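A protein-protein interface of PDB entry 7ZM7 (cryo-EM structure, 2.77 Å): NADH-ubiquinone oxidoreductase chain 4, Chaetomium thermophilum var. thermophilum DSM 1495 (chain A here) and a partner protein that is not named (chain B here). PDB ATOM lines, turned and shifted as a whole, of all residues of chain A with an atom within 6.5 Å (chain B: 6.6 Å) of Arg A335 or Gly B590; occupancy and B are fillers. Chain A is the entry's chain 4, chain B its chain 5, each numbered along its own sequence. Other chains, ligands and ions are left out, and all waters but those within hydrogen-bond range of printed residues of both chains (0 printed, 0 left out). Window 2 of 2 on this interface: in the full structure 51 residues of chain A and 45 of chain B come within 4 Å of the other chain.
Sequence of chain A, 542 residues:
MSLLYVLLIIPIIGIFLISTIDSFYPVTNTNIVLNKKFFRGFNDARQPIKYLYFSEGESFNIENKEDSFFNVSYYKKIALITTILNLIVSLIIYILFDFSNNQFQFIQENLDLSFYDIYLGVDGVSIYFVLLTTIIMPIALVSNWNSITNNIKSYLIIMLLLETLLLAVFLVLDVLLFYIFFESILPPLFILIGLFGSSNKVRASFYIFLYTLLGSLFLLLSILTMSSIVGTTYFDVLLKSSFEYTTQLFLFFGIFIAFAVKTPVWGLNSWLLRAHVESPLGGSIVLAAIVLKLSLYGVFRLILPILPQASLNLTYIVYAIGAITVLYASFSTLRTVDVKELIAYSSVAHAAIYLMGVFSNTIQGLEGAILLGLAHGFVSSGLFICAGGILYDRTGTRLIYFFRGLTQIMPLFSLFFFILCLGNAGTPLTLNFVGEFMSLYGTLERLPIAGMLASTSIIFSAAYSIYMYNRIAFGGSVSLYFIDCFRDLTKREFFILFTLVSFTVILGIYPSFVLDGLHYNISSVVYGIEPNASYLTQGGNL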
ATOM      1  N   SER A 330       2.681  18.317  22.975  1.00  0.00           N
ATOM      2  CA  SER A 330       1.919  18.294  21.737  1.00  0.00           C
ATOM      3  C   SER A 330       1.610  16.871  21.296  1.00  0.00           C
ATOM      4  O   SER A 330       0.526  16.606  20.772  1.00  0.00           O
ATOM      5  CB  SER A 330       2.679  19.033  20.648  1.00  0.00           C
ATOM      6  OG  SER A 330       2.784  20.408  20.939  1.00  0.00           O
ATOM      7  N   PHE A 331       2.557  15.948  21.476  1.00  0.00           N
ATOM      8  CA  PHE A 331       2.332  14.564  21.070  1.00  0.00           C
ATOM      9  C   PHE A 331       1.254  13.906  21.911  1.00  0.00           C
ATOM     10  O   PHE A 331       0.436  13.145  21.391  1.00  0.00           O
ATOM     11  CB  PHE A 331       3.625  13.760  21.159  1.00  0.00           C
ATOM     12  CG  PHE A 331       4.680  14.205  20.201  1.00  0.00           C
ATOM     13  CD1 PHE A 331       4.365  15.041  19.148  1.00  0.00           C
ATOM     14  CD2 PHE A 331       5.993  13.803  20.365  1.00  0.00           C
ATOM     15  CE1 PHE A 331       5.326  15.460  18.290  1.00  0.00           C
ATOM     16  CE2 PHE A 331       6.963  14.220  19.504  1.00  0.00           C
ATOM     17  CZ  PHE A 331       6.626  15.040  18.454  1.00  0.00           C
ATOM     18  N   SER A 332       1.240  14.178  23.209  1.00  0.00           N
ATOM     19  CA  SER A 332       0.269  13.541  24.080  1.00  0.00           C
ATOM     20  C   SER A 332      -1.035  14.310  24.195  1.00  0.00           C
ATOM     21  O   SER A 332      -1.984  13.793  24.785  1.00  0.00           O
ATOM     22  CB  SER A 332       0.875  13.313  25.462  1.00  0.00           C
ATOM     23  OG  SER A 332       1.336  14.507  26.022  1.00  0.00           O
ATOM     24  N   THR A 333      -1.118  15.511  23.638  1.00  0.00           N
ATOM     25  CA  THR A 333      -2.411  16.164  23.522  1.00  0.00           C
ATOM     26  C   THR A 333      -3.217  15.567  22.376  1.00  0.00           C
ATOM     27  O   THR A 333      -4.439  15.715  22.347  1.00  0.00           O
ATOM     28  CB  THR A 333      -2.222  17.678  23.341  1.00  0.00           C
ATOM     29  OG1 THR A 333      -1.360  18.162  24.366  1.00  0.00           O
ATOM     30  CG2 THR A 333      -3.528  18.425  23.500  1.00  0.00           C
ATOM     31  N   LEU A 334      -2.562  14.881  21.441  1.00  0.00           N
ATOM     32  CA  LEU A 334      -3.285  14.130  20.420  1.00  0.00           C
ATOM     33  C   LEU A 334      -4.023  12.929  20.980  1.00  0.00           C
ATOM     34  O   LEU A 334      -5.117  12.614  20.513  1.00  0.00           O
ATOM     35  CB  LEU A 334      -2.339  13.658  19.322  1.00  0.00           C
ATOM     36  CG  LEU A 334      -1.707  14.714  18.457  1.00  0.00           C
ATOM     37  CD1 LEU A 334      -0.704  14.069  17.539  1.00  0.00           C
ATOM     38  CD2 LEU A 334      -2.816  15.318  17.653  1.00  0.00           C
ATOM     39  N   ARG A 335      -3.446  12.231  21.951  1.00  0.00           N
ATOM     40  CA  ARG A 335      -3.971  10.944  22.377  1.00  0.00           C
ATOM     41  C   ARG A 335      -4.796  11.026  23.656  1.00  0.00           C
ATOM     42  O   ARG A 335      -4.977  10.015  24.334  1.00  0.00           O
ATOM     43  CB  ARG A 335      -2.826   9.949  22.531  1.00  0.00           C
ATOM     44  CG  ARG A 335      -2.108   9.651  21.225  1.00  0.00           C
ATOM     45  CD  ARG A 335      -2.959   8.910  20.215  1.00  0.00           C
ATOM     46  NE  ARG A 335      -3.348   7.591  20.685  1.00  0.00           N
ATOM     47  CZ  ARG A 335      -2.560   6.522  20.655  1.00  0.00           C
ATOM     48  NH1 ARG A 335      -1.333   6.617  20.190  1.00  0.00           N
ATOM     49  NH2 ARG A 335      -2.992   5.358  21.110  1.00  0.00           N
ATOM     50  N   THR A 336      -5.330  12.193  23.977  1.00  0.00           N
ATOM     51  CA  THR A 336      -6.095  12.383  25.200  1.00  0.00           C
ATOM     52  C   THR A 336      -7.580  12.153  24.938  1.00  0.00           C
ATOM     53  O   THR A 336      -8.168  12.789  24.062  1.00  0.00           O
ATOM     54  CB  THR A 336      -5.854  13.788  25.751  1.00  0.00           C
ATOM     55  OG1 THR A 336      -4.455  14.063  25.727  1.00  0.00           O
ATOM     56  CG2 THR A 336      -6.335  13.898  27.186  1.00  0.00           C
ATOM     57  N   VAL A 337      -8.197  11.280  25.731  1.00  0.00           N
ATOM     58  CA  VAL A 337      -9.621  10.908  25.488  1.00  0.00           C
ATOM     59  C   VAL A 337     -10.554  11.745  26.376  1.00  0.00           C
ATOM     60  O   VAL A 337     -11.765  11.680  26.153  1.00  0.00           O
ATOM     61  CB  VAL A 337      -9.821   9.394  25.713  1.00  0.00           C
ATOM     62  CG1 VAL A 337      -8.621   8.599  25.241  1.00  0.00           C
ATOM     63  CG2 VAL A 337     -10.103   9.071  27.173  1.00  0.00           C
ATOM     64  N   ASP A 338     -10.001  12.531  27.301  1.00  0.00           N
ATOM     65  CA  ASP A 338     -10.810  13.441  28.153  1.00  0.00           C
ATOM     66  C   ASP A 338     -10.788  14.829  27.504  1.00  0.00           C
ATOM     67  O   ASP A 338      -9.687  15.331  27.269  1.00  0.00           O
ATOM     68  CB  ASP A 338     -10.264  13.422  29.581  1.00  0.00           C
ATOM     69  CG  ASP A 338     -11.135  14.103  30.621  1.00  0.00           C
ATOM     70  OD1 ASP A 338     -11.428  15.302  30.459  1.00  0.00           O
ATOM     71  OD2 ASP A 338     -11.494  13.428  31.600  1.00  0.00           O
ATOM     72  N   LEU A 342      -7.735  17.454  27.504  1.00  0.00           N
ATOM     73  CA  LEU A 342      -7.113  17.883  26.230  1.00  0.00           C
ATOM     74  C   LEU A 342      -6.860  19.395  26.268  1.00  0.00           C
ATOM     75  O   LEU A 342      -5.800  19.825  25.807  1.00  0.00           O
ATOM     76  CB  LEU A 342      -8.065  17.469  25.107  1.00  0.00           C
ATOM     77  CG  LEU A 342      -7.426  17.066  23.780  1.00  0.00           C
ATOM     78  CD1 LEU A 342      -8.324  16.093  23.032  1.00  0.00           C
ATOM     79  CD2 LEU A 342      -7.130  18.287  22.919  1.00  0.00           C
ATOM     80  N   ARG A 471     -13.764  15.911  15.757  1.00  0.00           N
ATOM     81  CA  ARG A 471     -14.360  14.756  16.457  1.00  0.00           C
ATOM     82  C   ARG A 471     -15.672  15.129  17.156  1.00  0.00           C
ATOM     83  O   ARG A 471     -16.566  14.278  17.194  1.00  0.00           O
ATOM     84  CB  ARG A 471     -13.334  14.136  17.407  1.00  0.00           C
ATOM     85  CG  ARG A 471     -12.392  13.143  16.744  1.00  0.00           C
ATOM     86  CD  ARG A 471     -11.391  12.632  17.757  1.00  0.00           C
ATOM     87  NE  ARG A 471     -10.498  13.684  18.210  1.00  0.00           N
ATOM     88  CZ  ARG A 471      -9.609  13.544  19.183  1.00  0.00           C
ATOM     89  NH1 ARG A 471      -8.835  14.557  19.526  1.00  0.00           N
ATOM     90  NH2 ARG A 471      -9.505  12.391  19.818  1.00  0.00           N
ATOM     91  N   ILE B 585       3.688   9.426  14.577  1.00  0.00           N
ATOM     92  CA  ILE B 585       3.387  10.500  15.513  1.00  0.00           C
ATOM     93  C   ILE B 585       2.308  10.072  16.501  1.00  0.00           C
ATOM     94  O   ILE B 585       2.346  10.443  17.676  1.00  0.00           O
ATOM     95  CB  ILE B 585       2.990  11.771  14.745  1.00  0.00           C
ATOM     96  CG1 ILE B 585       4.206  12.360  14.051  1.00  0.00           C
ATOM     97  CG2 ILE B 585       2.432  12.791  15.681  1.00  0.00           C
ATOM     98  CD1 ILE B 585       5.250  12.851  15.005  1.00  0.00           C
ATOM     99  N   LEU B 586       1.328   9.294  16.048  1.00  0.00           N
ATOM    100  CA  LEU B 586       0.281   8.858  16.961  1.00  0.00           C
ATOM    101  C   LEU B 586       0.812   7.878  17.991  1.00  0.00           C
ATOM    102  O   LEU B 586       0.353   7.868  19.136  1.00  0.00           O
ATOM    103  CB  LEU B 586      -0.884   8.235  16.197  1.00  0.00           C
ATOM    104  CG  LEU B 586      -1.950   9.142  15.617  1.00  0.00           C
ATOM    105  CD1 LEU B 586      -2.600   9.825  16.783  1.00  0.00           C
ATOM    106  CD2 LEU B 586      -1.408  10.155  14.652  1.00  0.00           C
ATOM    107  N   ASN B 587       1.760   7.030  17.603  1.00  0.00           N
ATOM    108  CA  ASN B 587       2.344   6.096  18.553  1.00  0.00           C
ATOM    109  C   ASN B 587       3.356   6.772  19.462  1.00  0.00           C
ATOM    110  O   ASN B 587       3.529   6.348  20.606  1.00  0.00           O
ATOM    111  CB  ASN B 587       2.990   4.933  17.809  1.00  0.00           C
ATOM    112  CG  ASN B 587       2.054   4.305  16.801  1.00  0.00           C
ATOM    113  OD1 ASN B 587       0.878   4.669  16.717  1.00  0.00           O
ATOM    114  ND2 ASN B 587       2.569   3.371  16.016  1.00  0.00           N
ATOM    115  N   LEU B 588       4.059   7.792  18.971  1.00  0.00           N
ATOM    116  CA  LEU B 588       4.890   8.594  19.858  1.00  0.00           C
ATOM    117  C   LEU B 588       4.041   9.265  20.922  1.00  0.00           C
ATOM    118  O   LEU B 588       4.402   9.273  22.102  1.00  0.00           O
ATOM    119  CB  LEU B 588       5.663   9.651  19.075  1.00  0.00           C
ATOM    120  CG  LEU B 588       6.837   9.283  18.170  1.00  0.00           C
ATOM    121  CD1 LEU B 588       7.417  10.548  17.607  1.00  0.00           C
ATOM    122  CD2 LEU B 588       7.898   8.522  18.893  1.00  0.00           C
ATOM    123  N   GLY B 589       2.904   9.822  20.523  1.00  0.00           N
ATOM    124  CA  GLY B 589       2.010  10.416  21.494  1.00  0.00           C
ATOM    125  C   GLY B 589       1.469   9.404  22.477  1.00  0.00           C
ATOM    126  O   GLY B 589       1.291   9.709  23.658  1.00  0.00           O
ATOM    127  N   GLY B 590       1.197   8.188  22.005  1.00  0.00           N
ATOM    128  CA  GLY B 590       0.760   7.137  22.902  1.00  0.00           C
ATOM    129  C   GLY B 590       1.842   6.693  23.865  1.00  0.00           C
ATOM    130  O   GLY B 590       1.570   6.424  25.033  1.00  0.00           O
ATOM    131  N   GLN B 591       3.077   6.593  23.382  1.00  0.00           N
ATOM    132  CA  GLN B 591       4.183   6.175  24.236  1.00  0.00           C
ATOM    133  C   GLN B 591       4.457   7.195  25.330  1.00  0.00           C
ATOM    134  O   GLN B 591       4.719   6.828  26.479  1.00  0.00           O
ATOM    135  CB  GLN B 591       5.431   5.940  23.390  1.00  0.00           C
ATOM    136  CG  GLN B 591       5.560   4.514  22.946  1.00  0.00           C
ATOM    137  CD  GLN B 591       6.986   4.081  22.764  1.00  0.00           C
ATOM    138  OE1 GLN B 591       7.886   4.905  22.620  1.00  0.00           O
ATOM    139  NE2 GLN B 591       7.208   2.775  22.776  1.00  0.00           N
ATOM    140  N   ILE B 592       4.402   8.480  24.986  1.00  0.00           N
ATOM    141  CA  ILE B 592       4.595   9.526  25.980  1.00  0.00           C
ATOM    142  C   ILE B 592       3.457   9.525  26.987  1.00  0.00           C
ATOM    143  O   ILE B 592       3.677   9.714  28.187  1.00  0.00           O
ATOM    144  CB  ILE B 592       4.753  10.893  25.291  1.00  0.00           C
ATOM    145  CG1 ILE B 592       5.965  10.871  24.367  1.00  0.00           C
ATOM    146  CG2 ILE B 592       4.934  11.982  26.315  1.00  0.00           C
ATOM    147  CD1 ILE B 592       6.049  12.008  23.452  1.00  0.00           C
ATOM    148  N   THR B 593       2.225   9.319  26.524  1.00  0.00           N
ATOM    149  CA  THR B 593       1.082   9.305  27.430  1.00  0.00           C
ATOM    150  C   THR B 593       1.118   8.100  28.359  1.00  0.00           C
ATOM    151  O   THR B 593       0.905   8.233  29.568  1.00  0.00           O
ATOM    152  CB  THR B 593      -0.228   9.320  26.639  1.00  0.00           C
ATOM    153  OG1 THR B 593      -0.237  10.416  25.723  1.00  0.00           O
ATOM    154  CG2 THR B 593      -1.413   9.451  27.576  1.00  0.00           C
ATOM    155  N   LYS B 594       1.368   6.912  27.816  1.00  0.00           N
ATOM    156  CA  LYS B 594       1.252   5.710  28.633  1.00  0.00           C
ATOM    157  C   LYS B 594       2.515   5.432  29.431  1.00  0.00           C
ATOM    158  O   LYS B 594       2.455   5.214  30.642  1.00  0.00           O
ATOM    159  CB  LYS B 594       0.913   4.499  27.769  1.00  0.00           C
ATOM    160  CG  LYS B 594      -0.418   4.570  27.088  1.00  0.00           C
ATOM    161  CD  LYS B 594      -0.673   3.272  26.325  1.00  0.00           C
ATOM    162  CE  LYS B 594       0.195   3.082  25.088  1.00  0.00           C
ATOM    163  NZ  LYS B 594      -0.108   4.072  24.033  1.00  0.00           N
ATOM    164  N   ILE B 595       3.665   5.405  28.768  1.00  0.00           N
ATOM    165  CA  ILE B 595       4.871   4.952  29.440  1.00  0.00           C
ATOM    166  C   ILE B 595       5.438   6.021  30.356  1.00  0.00           C
ATOM    167  O   ILE B 595       6.038   5.697  31.385  1.00  0.00           O
ATOM    168  CB  ILE B 595       5.902   4.480  28.402  1.00  0.00           C
ATOM    169  CG1 ILE B 595       5.300   3.360  27.552  1.00  0.00           C
ATOM    170  CG2 ILE B 595       7.190   4.032  29.082  1.00  0.00           C
ATOM    171  CD1 ILE B 595       6.244   2.750  26.608  1.00  0.00           C
ATOM    172  N   LEU B 596       5.241   7.300  30.046  1.00  0.00           N
ATOM    173  CA  LEU B 596       5.891   8.350  30.813  1.00  0.00           C
ATOM    174  C   LEU B 596       4.920   9.113  31.699  1.00  0.00           C
ATOM    175  O   LEU B 596       5.070   9.083  32.920  1.00  0.00           O
ATOM    176  CB  LEU B 596       6.624   9.327  29.886  1.00  0.00           C
ATOM    177  CG  LEU B 596       7.384   8.765  28.689  1.00  0.00           C
ATOM    178  CD1 LEU B 596       8.031   9.873  27.941  1.00  0.00           C
ATOM    179  CD2 LEU B 596       8.413   7.771  29.110  1.00  0.00           C
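Among the printed residues, pairs that only touch across the chains: Ser A332 with Thr B593, Phe A331 with Gly B589, Phe A331 with Ile B592, Arg A335 with Gly B589, Leu A334 with Ile B585 and Ser A332 with Gly B589.
Of chain B, only Leu B586, Gly B589 and Gly B590 come within 4 Å of Arg A335.
Gly B590 touches one residue of chain A.
Of the printed residues of chain A, Thr B593 touches Ser A332 (3.1 Å).
Of the printed residues of chain B, Leu A334 touches Ile B585.
Lys B594 touches none of the printed residues of chain A.
Leu A342 touches none of the printed residues of chain B.
The nearest printed residue of chain B that does not touch Leu A334 is Leu B586 (4.6 Å).
The guanidinium group of Arg A335 sits close to the backbone carbonyl oxygen of Leu B586.
NH1 of Arg A335 lies close to N of Gly B590, at 3.5 Å.
Of the 11 printed residues of chain A, 4 touch a printed residue of chain B.
Printed residues of chain A that touch a printed residue of chain B: Phe A331, Ser A332, Leu A334 and Arg A335.
Hydrophobic or aromatic side chains of chain A within 4 Å of the printed part of chain B: Phe A331 and Leu A334.
The backbone carbonyl oxygen of Ser A332 sits at hydrogen-bond distance from the side-chain hydroxyl of Thr A336 (2.7 Å).
The side-chain hydroxyl (OG1) of Thr B593 sits at hydrogen-bond distance from the backbone carbonyl oxygen (O) of Gly B589 (2.7 Å).
The side-chain amino group of Lys B594 is in hydrogen-bond range of the backbone carbonyl oxygen of Gly B590 (3.1 Å).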
